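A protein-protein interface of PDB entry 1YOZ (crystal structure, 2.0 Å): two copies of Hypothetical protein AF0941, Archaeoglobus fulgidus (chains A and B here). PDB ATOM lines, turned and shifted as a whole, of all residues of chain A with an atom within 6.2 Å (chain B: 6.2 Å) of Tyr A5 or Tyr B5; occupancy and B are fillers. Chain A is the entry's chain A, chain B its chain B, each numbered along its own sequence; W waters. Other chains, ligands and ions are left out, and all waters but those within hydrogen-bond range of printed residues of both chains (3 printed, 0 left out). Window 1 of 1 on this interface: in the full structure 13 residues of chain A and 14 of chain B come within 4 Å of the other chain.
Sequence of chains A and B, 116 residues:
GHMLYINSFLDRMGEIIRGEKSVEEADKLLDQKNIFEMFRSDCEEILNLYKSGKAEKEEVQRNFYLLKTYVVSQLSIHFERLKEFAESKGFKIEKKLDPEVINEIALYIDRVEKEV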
ATOM      1  N   HIS A   2      10.873  24.982   5.512  1.00  0.00           N
ATOM      2  CA  HIS A   2       9.626  24.298   5.469  1.00  0.00           C
ATOM      3  C   HIS A   2       8.739  24.358   6.714  1.00  0.00           C
ATOM      4  O   HIS A   2       7.732  23.680   6.714  1.00  0.00           O
ATOM      5  CB  HIS A   2       9.836  22.852   4.973  1.00  0.00           C
ATOM      6  CG  HIS A   2      10.071  21.839   6.058  1.00  0.00           C
ATOM      7  ND1 HIS A   2      11.305  21.622   6.627  1.00  0.00           N
ATOM      8  CD2 HIS A   2       9.222  20.957   6.652  1.00  0.00           C
ATOM      9  CE1 HIS A   2      11.215  20.647   7.518  1.00  0.00           C
ATOM     10  NE2 HIS A   2       9.960  20.226   7.551  1.00  0.00           N
ATOM     11  N   MET A   3       9.074  25.159   7.722  1.00  0.00           N
ATOM     12  CA  MET A   3       8.257  25.183   8.933  1.00  0.00           C
ATOM     13  C   MET A   3       7.828  26.559   9.342  1.00  0.00           C
ATOM     14  O   MET A   3       6.718  26.746   9.796  1.00  0.00           O
ATOM     15  CB  MET A   3       9.050  24.520  10.114  1.00  0.00           C
ATOM     16  CG  MET A   3       9.260  23.004   9.967  1.00  0.00           C
ATOM     17  SD  MET A   3      10.355  22.309  11.293  1.00  0.00           S
ATOM     18  CE  MET A   3       9.927  23.255  12.612  1.00  0.00           C
ATOM     19  N   LEU A   4       8.705  27.560   9.175  1.00  0.00           N
ATOM     20  CA  LEU A   4       8.477  28.875   9.713  1.00  0.00           C
ATOM     21  C   LEU A   4       7.456  29.728   8.930  1.00  0.00           C
ATOM     22  O   LEU A   4       7.630  29.956   7.722  1.00  0.00           O
ATOM     23  CB  LEU A   4       9.820  29.637   9.819  1.00  0.00           C
ATOM     24  CG  LEU A   4       9.669  31.040  10.417  1.00  0.00           C
ATOM     25  CD1 LEU A   4       9.377  30.995  11.967  1.00  0.00           C
ATOM     26  CD2 LEU A   4      10.986  31.836  10.107  1.00  0.00           C
ATOM     27  N   TYR A   5       6.437  30.217   9.624  1.00  0.00           N
ATOM     28  CA  TYR A   5       5.414  31.138   9.034  1.00  0.00           C
ATOM     29  C   TYR A   5       4.718  32.020  10.054  1.00  0.00           C
ATOM     30  O   TYR A   5       3.602  31.707  10.546  1.00  0.00           O
ATOM     31  CB  TYR A   5       4.402  30.354   8.163  1.00  0.00           C
ATOM     32  CG  TYR A   5       3.360  31.178   7.425  1.00  0.00           C
ATOM     33  CD1 TYR A   5       3.711  32.297   6.686  1.00  0.00           C
ATOM     34  CD2 TYR A   5       2.032  30.806   7.443  1.00  0.00           C
ATOM     35  CE1 TYR A   5       2.741  33.031   5.978  1.00  0.00           C
ATOM     36  CE2 TYR A   5       1.024  31.557   6.732  1.00  0.00           C
ATOM     37  CZ  TYR A   5       1.399  32.642   5.985  1.00  0.00           C
ATOM     38  OH  TYR A   5       0.409  33.337   5.280  1.00  0.00           O
ATOM     39  N   ILE A   6       5.369  33.142  10.403  1.00  0.00           N
ATOM     40  CA  ILE A   6       4.704  34.146  11.217  1.00  0.00           C
ATOM     41  C   ILE A   6       3.784  34.895  10.278  1.00  0.00           C
ATOM     42  O   ILE A   6       4.185  35.216   9.139  1.00  0.00           O
ATOM     43  CB  ILE A   6       5.733  35.097  11.897  1.00  0.00           C
ATOM     44  CG1 ILE A   6       6.598  34.271  12.890  1.00  0.00           C
ATOM     45  CG2 ILE A   6       5.051  36.414  12.495  1.00  0.00           C
ATOM     46  CD1 ILE A   6       7.805  35.043  13.414  1.00  0.00           C
ATOM     47  N   ASN A   7       2.554  35.124  10.729  1.00  0.00           N
ATOM     48  CA  ASN A   7       1.575  35.986  10.079  1.00  0.00           C
ATOM     49  C   ASN A   7       0.501  36.333  11.129  1.00  0.00           C
ATOM     50  O   ASN A   7      -0.407  35.500  11.417  1.00  0.00           O
ATOM     51  CB  ASN A   7       0.983  35.337   8.812  1.00  0.00           C
ATOM     52  CG  ASN A   7       0.043  36.273   8.042  1.00  0.00           C
ATOM     53  OD1 ASN A   7      -0.458  37.268   8.567  1.00  0.00           O
ATOM     54  ND2 ASN A   7      -0.229  35.926   6.789  1.00  0.00           N
ATOM     55  N   LEU A  10      -3.364  37.021   9.781  1.00  0.00           N
ATOM     56  CA  LEU A  10      -3.999  35.741   9.539  1.00  0.00           C
ATOM     57  C   LEU A  10      -4.424  35.032  10.860  1.00  0.00           C
ATOM     58  O   LEU A  10      -5.574  34.643  11.010  1.00  0.00           O
ATOM     59  CB  LEU A  10      -3.058  34.849   8.725  1.00  0.00           C
ATOM     60  CG  LEU A  10      -3.518  33.403   8.363  1.00  0.00           C
ATOM     61  CD1 LEU A  10      -4.894  33.342   7.625  1.00  0.00           C
ATOM     62  CD2 LEU A  10      -2.421  32.744   7.526  1.00  0.00           C
ATOM     63  N   ASP A  11      -3.500  34.890  11.804  1.00  0.00           N
ATOM     64  CA  ASP A  11      -3.837  34.252  13.087  1.00  0.00           C
ATOM     65  C   ASP A  11      -4.929  35.013  13.873  1.00  0.00           C
ATOM     66  O   ASP A  11      -5.802  34.391  14.469  1.00  0.00           O
ATOM     67  CB  ASP A  11      -2.613  34.165  13.954  1.00  0.00           C
ATOM     68  CG  ASP A  11      -1.637  33.070  13.504  1.00  0.00           C
ATOM     69  OD1 ASP A  11      -1.974  32.177  12.700  1.00  0.00           O
ATOM     70  OD2 ASP A  11      -0.517  33.115  13.998  1.00  0.00           O
ATOM     71  N   GLU A  59      14.560  29.150   6.399  1.00  0.00           N
ATOM     72  CA  GLU A  59      13.245  29.183   7.020  1.00  0.00           C
ATOM     73  C   GLU A  59      12.741  30.625   7.005  1.00  0.00           C
ATOM     74  O   GLU A  59      11.553  30.903   6.774  1.00  0.00           O
ATOM     75  CB  GLU A  59      13.302  28.654   8.459  1.00  0.00           C
ATOM     76  CG  GLU A  59      13.524  27.103   8.572  1.00  0.00           C
ATOM     77  CD  GLU A  59      12.326  26.288   8.111  1.00  0.00           C
ATOM     78  OE1 GLU A  59      11.256  26.880   7.863  1.00  0.00           O
ATOM     79  OE2 GLU A  59      12.459  25.042   7.999  1.00  0.00           O
ATOM     80  N   ARG A  62      11.628  31.410   3.493  1.00  0.00           N
ATOM     81  CA  ARG A  62      10.338  30.771   3.190  1.00  0.00           C
ATOM     82  C   ARG A  62       9.236  31.629   3.782  1.00  0.00           C
ATOM     83  O   ARG A  62       8.182  31.832   3.164  1.00  0.00           O
ATOM     84  CB  ARG A  62      10.322  29.331   3.759  1.00  0.00           C
ATOM     85  CG  ARG A  62       9.130  28.470   3.378  1.00  0.00           C
ATOM     86  CD  ARG A  62       8.351  28.054   4.614  1.00  0.00           C
ATOM     87  NE  ARG A  62       7.258  27.129   4.291  1.00  0.00           N
ATOM     88  CZ  ARG A  62       6.313  26.802   5.170  1.00  0.00           C
ATOM     89  NH1 ARG A  62       6.307  27.366   6.382  1.00  0.00           N
ATOM     90  NH2 ARG A  62       5.373  25.939   4.825  1.00  0.00           N
ATOM     91  N   ASN A  63       9.455  32.100   5.007  1.00  0.00           N
ATOM     92  CA  ASN A  63       8.442  32.897   5.676  1.00  0.00           C
ATOM     93  C   ASN A  63       8.204  34.200   4.914  1.00  0.00           C
ATOM     94  O   ASN A  63       7.082  34.671   4.838  1.00  0.00           O
ATOM     95  CB  ASN A  63       8.828  33.195   7.114  1.00  0.00           C
ATOM     96  CG  ASN A  63       7.661  33.744   7.942  1.00  0.00           C
ATOM     97  OD1 ASN A  63       6.589  34.177   7.439  1.00  0.00           O
ATOM     98  ND2 ASN A  63       7.874  33.746   9.226  1.00  0.00           N
ATOM     99  N   LEU A  66       6.213  33.367   1.771  1.00  0.00           N
ATOM    100  CA  LEU A  66       4.809  33.110   2.096  1.00  0.00           C
ATOM    101  C   LEU A  66       4.087  34.365   2.481  1.00  0.00           C
ATOM    102  O   LEU A  66       2.938  34.512   2.120  1.00  0.00           O
ATOM    103  CB  LEU A  66       4.673  32.085   3.239  1.00  0.00           C
ATOM    104  CG  LEU A  66       5.007  30.642   2.909  1.00  0.00           C
ATOM    105  CD1 LEU A  66       4.581  29.738   4.117  1.00  0.00           C
ATOM    106  CD2 LEU A  66       4.317  30.199   1.598  1.00  0.00           C
ATOM    107  N   LEU A  67       4.745  35.233   3.263  1.00  0.00           N
ATOM    108  CA  LEU A  67       4.120  36.470   3.758  1.00  0.00           C
ATOM    109  C   LEU A  67       3.812  37.394   2.573  1.00  0.00           C
ATOM    110  O   LEU A  67       2.711  37.888   2.458  1.00  0.00           O
ATOM    111  CB  LEU A  67       5.040  37.188   4.733  1.00  0.00           C
ATOM    112  CG  LEU A  67       4.438  38.164   5.752  1.00  0.00           C
ATOM    113  CD1 LEU A  67       3.428  37.454   6.606  1.00  0.00           C
ATOM    114  CD2 LEU A  67       5.589  38.862   6.563  1.00  0.00           C
ATOM    115  N   TYR A  70       0.989  35.823   0.627  1.00  0.00           N
ATOM    116  CA  TYR A  70      -0.275  36.092   1.365  1.00  0.00           C
ATOM    117  C   TYR A  70      -0.815  37.528   1.101  1.00  0.00           C
ATOM    118  O   TYR A  70      -2.004  37.712   0.830  1.00  0.00           O
ATOM    119  CB  TYR A  70      -0.110  35.892   2.897  1.00  0.00           C
ATOM    120  CG  TYR A  70      -1.377  36.175   3.650  1.00  0.00           C
ATOM    121  CD1 TYR A  70      -2.399  35.182   3.704  1.00  0.00           C
ATOM    122  CD2 TYR A  70      -1.599  37.426   4.250  1.00  0.00           C
ATOM    123  CE1 TYR A  70      -3.590  35.438   4.340  1.00  0.00           C
ATOM    124  CE2 TYR A  70      -2.844  37.719   4.950  1.00  0.00           C
ATOM    125  CZ  TYR A  70      -3.812  36.683   4.952  1.00  0.00           C
ATOM    126  OH  TYR A  70      -5.020  36.877   5.534  1.00  0.00           O
ATOM    127  N   HIS B   2       2.506  32.635  16.621  1.00  0.00           N
ATOM    128  CA  HIS B   2       2.615  31.205  16.399  1.00  0.00           C
ATOM    129  C   HIS B   2       3.514  31.213  15.159  1.00  0.00           C
ATOM    130  O   HIS B   2       3.495  32.172  14.362  1.00  0.00           O
ATOM    131  CB  HIS B   2       1.313  30.545  16.050  1.00  0.00           C
ATOM    132  CG  HIS B   2       0.373  30.411  17.207  1.00  0.00           C
ATOM    133  ND1 HIS B   2       0.717  29.770  18.378  1.00  0.00           N
ATOM    134  CD2 HIS B   2      -0.917  30.797  17.350  1.00  0.00           C
ATOM    135  CE1 HIS B   2      -0.310  29.798  19.211  1.00  0.00           C
ATOM    136  NE2 HIS B   2      -1.318  30.401  18.608  1.00  0.00           N
ATOM    137  N   MET B   3       4.326  30.186  15.005  1.00  0.00           N
ATOM    138  CA  MET B   3       5.347  30.225  13.974  1.00  0.00           C
ATOM    139  C   MET B   3       5.228  29.029  13.053  1.00  0.00           C
ATOM    140  O   MET B   3       5.583  29.119  11.886  1.00  0.00           O
ATOM    141  CB  MET B   3       6.779  30.287  14.616  1.00  0.00           C
ATOM    142  CG  MET B   3       7.138  31.586  15.400  1.00  0.00           C
ATOM    143  SD  MET B   3       8.523  31.390  16.623  1.00  0.00           S
ATOM    144  CE  MET B   3       9.523  30.465  15.572  1.00  0.00           C
ATOM    145  N   LEU B   4       4.688  27.910  13.559  1.00  0.00           N
ATOM    146  CA  LEU B   4       4.782  26.670  12.832  1.00  0.00           C
ATOM    147  C   LEU B   4       3.730  26.545  11.759  1.00  0.00           C
ATOM    148  O   LEU B   4       2.538  26.789  11.997  1.00  0.00           O
ATOM    149  CB  LEU B   4       4.734  25.458  13.813  1.00  0.00           C
ATOM    150  CG  LEU B   4       4.812  24.026  13.263  1.00  0.00           C
ATOM    151  CD1 LEU B   4       6.150  23.578  12.607  1.00  0.00           C
ATOM    152  CD2 LEU B   4       4.397  22.980  14.357  1.00  0.00           C
ATOM    153  N   TYR B   5       4.166  26.159  10.575  1.00  0.00           N
ATOM    154  CA  TYR B   5       3.218  25.855   9.483  1.00  0.00           C
ATOM    155  C   TYR B   5       3.922  25.018   8.466  1.00  0.00           C
ATOM    156  O   TYR B   5       4.504  25.537   7.490  1.00  0.00           O
ATOM    157  CB  TYR B   5       2.631  27.133   8.836  1.00  0.00           C
ATOM    158  CG  TYR B   5       1.675  26.891   7.661  1.00  0.00           C
ATOM    159  CD1 TYR B   5       1.843  27.544   6.432  1.00  0.00           C
ATOM    160  CD2 TYR B   5       0.600  26.021   7.781  1.00  0.00           C
ATOM    161  CE1 TYR B   5       0.933  27.374   5.400  1.00  0.00           C
ATOM    162  CE2 TYR B   5      -0.307  25.828   6.739  1.00  0.00           C
ATOM    163  CZ  TYR B   5      -0.150  26.501   5.565  1.00  0.00           C
ATOM    164  OH  TYR B   5      -1.022  26.239   4.534  1.00  0.00           O
ATOM    165  N   ILE B   6       3.891  23.711   8.716  1.00  0.00           N
ATOM    166  CA  ILE B   6       4.252  22.720   7.745  1.00  0.00           C
ATOM    167  C   ILE B   6       3.130  22.541   6.685  1.00  0.00           C
ATOM    168  O   ILE B   6       1.960  22.425   7.023  1.00  0.00           O
ATOM    169  CB  ILE B   6       4.582  21.350   8.463  1.00  0.00           C
ATOM    170  CG1 ILE B   6       5.866  21.482   9.311  1.00  0.00           C
ATOM    171  CG2 ILE B   6       4.694  20.241   7.466  1.00  0.00           C
ATOM    172  CD1 ILE B   6       6.162  20.286  10.288  1.00  0.00           C
ATOM    173  N   ASN B   7       3.510  22.556   5.396  1.00  0.00           N
ATOM    174  CA  ASN B   7       2.635  22.258   4.286  1.00  0.00           C
ATOM    175  C   ASN B   7       3.527  21.982   3.089  1.00  0.00           C
ATOM    176  O   ASN B   7       4.035  22.914   2.441  1.00  0.00           O
ATOM    177  CB  ASN B   7       1.682  23.456   3.989  1.00  0.00           C
ATOM    178  CG  ASN B   7       0.676  23.148   2.923  1.00  0.00           C
ATOM    179  OD1 ASN B   7       0.870  22.245   2.116  1.00  0.00           O
ATOM    180  ND2 ASN B   7      -0.383  23.964   2.846  1.00  0.00           N
ATOM    181  N   LEU B  10       2.174  23.010  -0.531  1.00  0.00           N
ATOM    182  CA  LEU B  10       2.384  24.452  -0.741  1.00  0.00           C
ATOM    183  C   LEU B  10       3.836  24.777  -1.065  1.00  0.00           C
ATOM    184  O   LEU B  10       4.123  25.475  -2.029  1.00  0.00           O
ATOM    185  CB  LEU B  10       1.860  25.259   0.459  1.00  0.00           C
ATOM    186  CG  LEU B  10       2.072  26.777   0.374  1.00  0.00           C
ATOM    187  CD1 LEU B  10       1.215  27.430  -0.676  1.00  0.00           C
ATOM    188  CD2 LEU B  10       1.822  27.326   1.738  1.00  0.00           C
ATOM    189  N   ASP B  11       4.778  24.206  -0.321  1.00  0.00           N
ATOM    190  CA  ASP B  11       6.180  24.497  -0.593  1.00  0.00           C
ATOM    191  C   ASP B  11       6.635  23.930  -1.938  1.00  0.00           C
ATOM    192  O   ASP B  11       7.357  24.602  -2.674  1.00  0.00           O
ATOM    193  CB  ASP B  11       7.100  23.961   0.512  1.00  0.00           C
ATOM    194  CG  ASP B  11       6.994  24.739   1.820  1.00  0.00           C
ATOM    195  OD1 ASP B  11       6.829  25.991   1.855  1.00  0.00           O
ATOM    196  OD2 ASP B  11       7.091  24.076   2.843  1.00  0.00           O
ATOM    197  N   GLU B  59       0.829  25.650  19.105  1.00  0.00           N
ATOM    198  CA  GLU B  59       1.522  25.782  17.822  1.00  0.00           C
ATOM    199  C   GLU B  59       1.044  24.712  16.868  1.00  0.00           C
ATOM    200  O   GLU B  59       0.840  24.984  15.691  1.00  0.00           O
ATOM    201  CB  GLU B  59       3.046  25.616  17.904  1.00  0.00           C
ATOM    202  CG  GLU B  59       3.873  26.761  18.406  1.00  0.00           C
ATOM    203  CD  GLU B  59       4.043  27.879  17.429  1.00  0.00           C
ATOM    204  OE1 GLU B  59       4.799  27.768  16.436  1.00  0.00           O
ATOM    205  OE2 GLU B  59       3.463  28.908  17.706  1.00  0.00           O
ATOM    206  N   ARG B  62      -2.526  25.548  15.708  1.00  0.00           N
ATOM    207  CA  ARG B  62      -2.440  26.561  14.648  1.00  0.00           C
ATOM    208  C   ARG B  62      -2.061  25.927  13.307  1.00  0.00           C
ATOM    209  O   ARG B  62      -2.755  26.101  12.328  1.00  0.00           O
ATOM    210  CB  ARG B  62      -1.417  27.600  15.102  1.00  0.00           C
ATOM    211  CG  ARG B  62      -1.400  28.877  14.276  1.00  0.00           C
ATOM    212  CD  ARG B  62      -0.319  28.810  13.225  1.00  0.00           C
ATOM    213  NE  ARG B  62      -0.172  30.111  12.582  1.00  0.00           N
ATOM    214  CZ  ARG B  62       0.888  30.497  11.877  1.00  0.00           C
ATOM    215  NH1 ARG B  62       1.897  29.649  11.667  1.00  0.00           N
ATOM    216  NH2 ARG B  62       0.884  31.714  11.320  1.00  0.00           N
ATOM    217  N   ASN B  63      -0.999  25.110  13.261  1.00  0.00           N
ATOM    218  CA  ASN B  63      -0.647  24.441  11.994  1.00  0.00           C
ATOM    219  C   ASN B  63      -1.791  23.593  11.403  1.00  0.00           C
ATOM    220  O   ASN B  63      -2.019  23.579  10.191  1.00  0.00           O
ATOM    221  CB  ASN B  63       0.625  23.579  12.208  1.00  0.00           C
ATOM    222  CG  ASN B  63       1.338  23.172  10.903  1.00  0.00           C
ATOM    223  OD1 ASN B  63       2.521  22.845  10.962  1.00  0.00           O
ATOM    224  ND2 ASN B  63       0.651  23.184   9.748  1.00  0.00           N
ATOM    225  N   LEU B  66      -4.523  25.957   9.969  1.00  0.00           N
ATOM    226  CA  LEU B  66      -4.116  26.501   8.678  1.00  0.00           C
ATOM    227  C   LEU B  66      -4.095  25.416   7.605  1.00  0.00           C
ATOM    228  O   LEU B  66      -4.418  25.668   6.437  1.00  0.00           O
ATOM    229  CB  LEU B  66      -2.728  27.190   8.780  1.00  0.00           C
ATOM    230  CG  LEU B  66      -2.493  28.462   9.628  1.00  0.00           C
ATOM    231  CD1 LEU B  66      -1.103  29.060   9.431  1.00  0.00           C
ATOM    232  CD2 LEU B  66      -3.535  29.447   9.219  1.00  0.00           C
ATOM    233  N   LEU B  67      -3.687  24.213   7.972  1.00  0.00           N
ATOM    234  CA  LEU B  67      -3.550  23.143   6.993  1.00  0.00           C
ATOM    235  C   LEU B  67      -4.945  22.676   6.546  1.00  0.00           C
ATOM    236  O   LEU B  67      -5.208  22.480   5.369  1.00  0.00           O
ATOM    237  CB  LEU B  67      -2.715  21.973   7.615  1.00  0.00           C
ATOM    238  CG  LEU B  67      -2.163  20.959   6.624  1.00  0.00           C
ATOM    239  CD1 LEU B  67      -1.033  21.538   5.799  1.00  0.00           C
ATOM    240  CD2 LEU B  67      -1.727  19.650   7.312  1.00  0.00           C
ATOM    241  N   TYR B  70      -6.313  25.429   4.479  1.00  0.00           N
ATOM    242  CA  TYR B  70      -5.635  25.390   3.177  1.00  0.00           C
ATOM    243  C   TYR B  70      -6.290  24.361   2.313  1.00  0.00           C
ATOM    244  O   TYR B  70      -6.543  24.614   1.129  1.00  0.00           O
ATOM    245  CB  TYR B  70      -4.137  25.006   3.302  1.00  0.00           C
ATOM    246  CG  TYR B  70      -3.434  24.944   1.957  1.00  0.00           C
ATOM    247  CD1 TYR B  70      -2.836  26.085   1.400  1.00  0.00           C
ATOM    248  CD2 TYR B  70      -3.347  23.752   1.237  1.00  0.00           C
ATOM    249  CE1 TYR B  70      -2.178  26.028   0.169  1.00  0.00           C
ATOM    250  CE2 TYR B  70      -2.697  23.716  -0.016  1.00  0.00           C
ATOM    251  CZ  TYR B  70      -2.118  24.854  -0.526  1.00  0.00           C
ATOM    252  OH  TYR B  70      -1.512  24.852  -1.757  1.00  0.00           O
HETATM  253  O   HOH W   1       0.099  33.949  16.501  1.00  0.00           O
HETATM  254  O   HOH W   2       1.860  34.528  13.471  1.00  0.00           O
HETATM  255  O   HOH W   3       6.288  22.522   4.710  1.00  0.00           O
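The backbone carbonyl oxygen (O) of Met A3 is in hydrogen-bond range of the backbone NH (N) of Tyr B5. The guanidinium group (NE) of Arg A62 is in salt-bridge range of the side-chain carboxylate (OD1) of Asp B11, at 2.7 Å. O of Met A3 lies close to O of Met B3 (3.4 Å). The side-chain carboxylate of Asp A11 lies within salt-bridge range of the guanidinium group of Arg B62, at 2.7 Å. O of Tyr B5 lies within hydrogen-bond range of NH1 of Arg A62, at 2.8 Å. The backbone NH (N) of Tyr A5 lies within hydrogen-bond range of the backbone carbonyl oxygen (O) of Met B3. The guanidinium group of Arg B62 is in hydrogen-bond range of the backbone carbonyl oxygen of Tyr A5, 2.8 Å away.
NH1 of Arg A62 lies close to O of Met A3, 3.5 Å away. The side-chain carboxylate (OE1) of Glu B59 is in hydrogen-bond range of the backbone NH (N) of Met B3 (2.8 Å). ND2 of Asn A7 sits at hydrogen-bond distance from OH of Tyr A5 (3.1 Å). The side-chain amide oxygen (OD1) of Asn B7 sits at hydrogen-bond distance from the backbone NH (N) of Leu B10, 3.0 Å away. The backbone carbonyl oxygen (O) of Leu A4 lies within hydrogen-bond range of the guanidinium group (NH1) of Arg A62 (3.2 Å). The backbone NH of Ile A6 sits close to the side-chain amide nitrogen of Asn A63.
His A2 touches Tyr B5 (O to O, 3.8 Å). His A2 touches Ile B6. Met B3 touches Leu A4 (O to C, 3.6 Å). Tyr A5 touches Tyr B5. CA of Ile A6 touches O of His B2, at 3.9 Å. Arg B62 touches Asn A7 (NH2 to N, 3.8 Å). Leu A10 touches Leu B66. OD2 of Asp A11 touches CB of His B2, at 3.8 Å. N of Asn B7 touches NH2 of Arg A62, 3.9 Å away. CD2 of Leu A66 touches CD2 of Leu B10, 3.8 Å away.
Printed residues of chain B within 4 Å of Met A3: Met B3 (3.4 Å), Leu B4 (3.6 Å), Tyr B5 (2.7 Å) and Ile B6 (3.8 Å). Of chain B, only His B2 (3.8 Å), Met B3 (2.7 Å), Tyr B5 (3.4 Å) and Arg B62 (2.8 Å) come within 4 Å of Tyr A5. Printed residues of chain B within 4 Å of Ile A6: His B2 (3.9 Å) and Met B3 (3.7 Å). Of the printed residues of chain B, Arg A62 touches Tyr B5, Asn B7 and Asp B11. Tyr B5 touches just these residues of chain A: His A2 (3.8 Å), Met A3 (2.7 Å), Tyr A5 (3.4 Å) and Arg A62 (2.8 Å). Glu B59 touches none of the printed residues of chain A. Of the printed residues of chain A, Leu B66 touches Leu A10 (3.9 Å). The nearest residue of chain B that does not touch Tyr A5 is Leu B66 (4.1 Å). The nearest residue of chain A that does not touch Tyr B5 is Leu A66 (4.2 Å).
Of the 14 printed residues of chain B, 10 touch a printed residue of chain A. Among the printed residues, 22 pairs touch across the chains. Among the printed residues, Asp or Glu carboxylates within 4 Å of a Lys or Arg side-chain nitrogen of the other chain: Asp A11 with Arg B62 (2.7 Å) and Arg A62 with Asp B11 (2.7 Å).
His A2 touches Ile B6, and with the chains exchanged Ile A6 touches His B2. His A2 touches Asp B11, and with the chains exchanged Asp A11 touches His B2. Met A3 touches its own counterpart, Met B3. Tyr A5 touches its own counterpart, Tyr B5. 14 positions are printed for both chains. Of the 22 pairs that touch across the chains among the printed residues, 22 have their exchanged pair printed and touching as well.
Water W3 lies within hydrogen-bond range of OD2 of Asp B11 (2.6 Å), O of His A2 (2.7 Å) and N of Asn B7 (2.9 Å). Water W1 bridges OD2 of Asp A11 (2.7 Å) and N of His B2 (2.7 Å). Water W2 lies within hydrogen-bond range of the side-chain carboxylate (OD2) of Asp A11 (2.8 Å), the backbone NH (N) of Asn A7 (2.9 Å) and the backbone carbonyl oxygen (O) of His B2 (3.0 Å).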
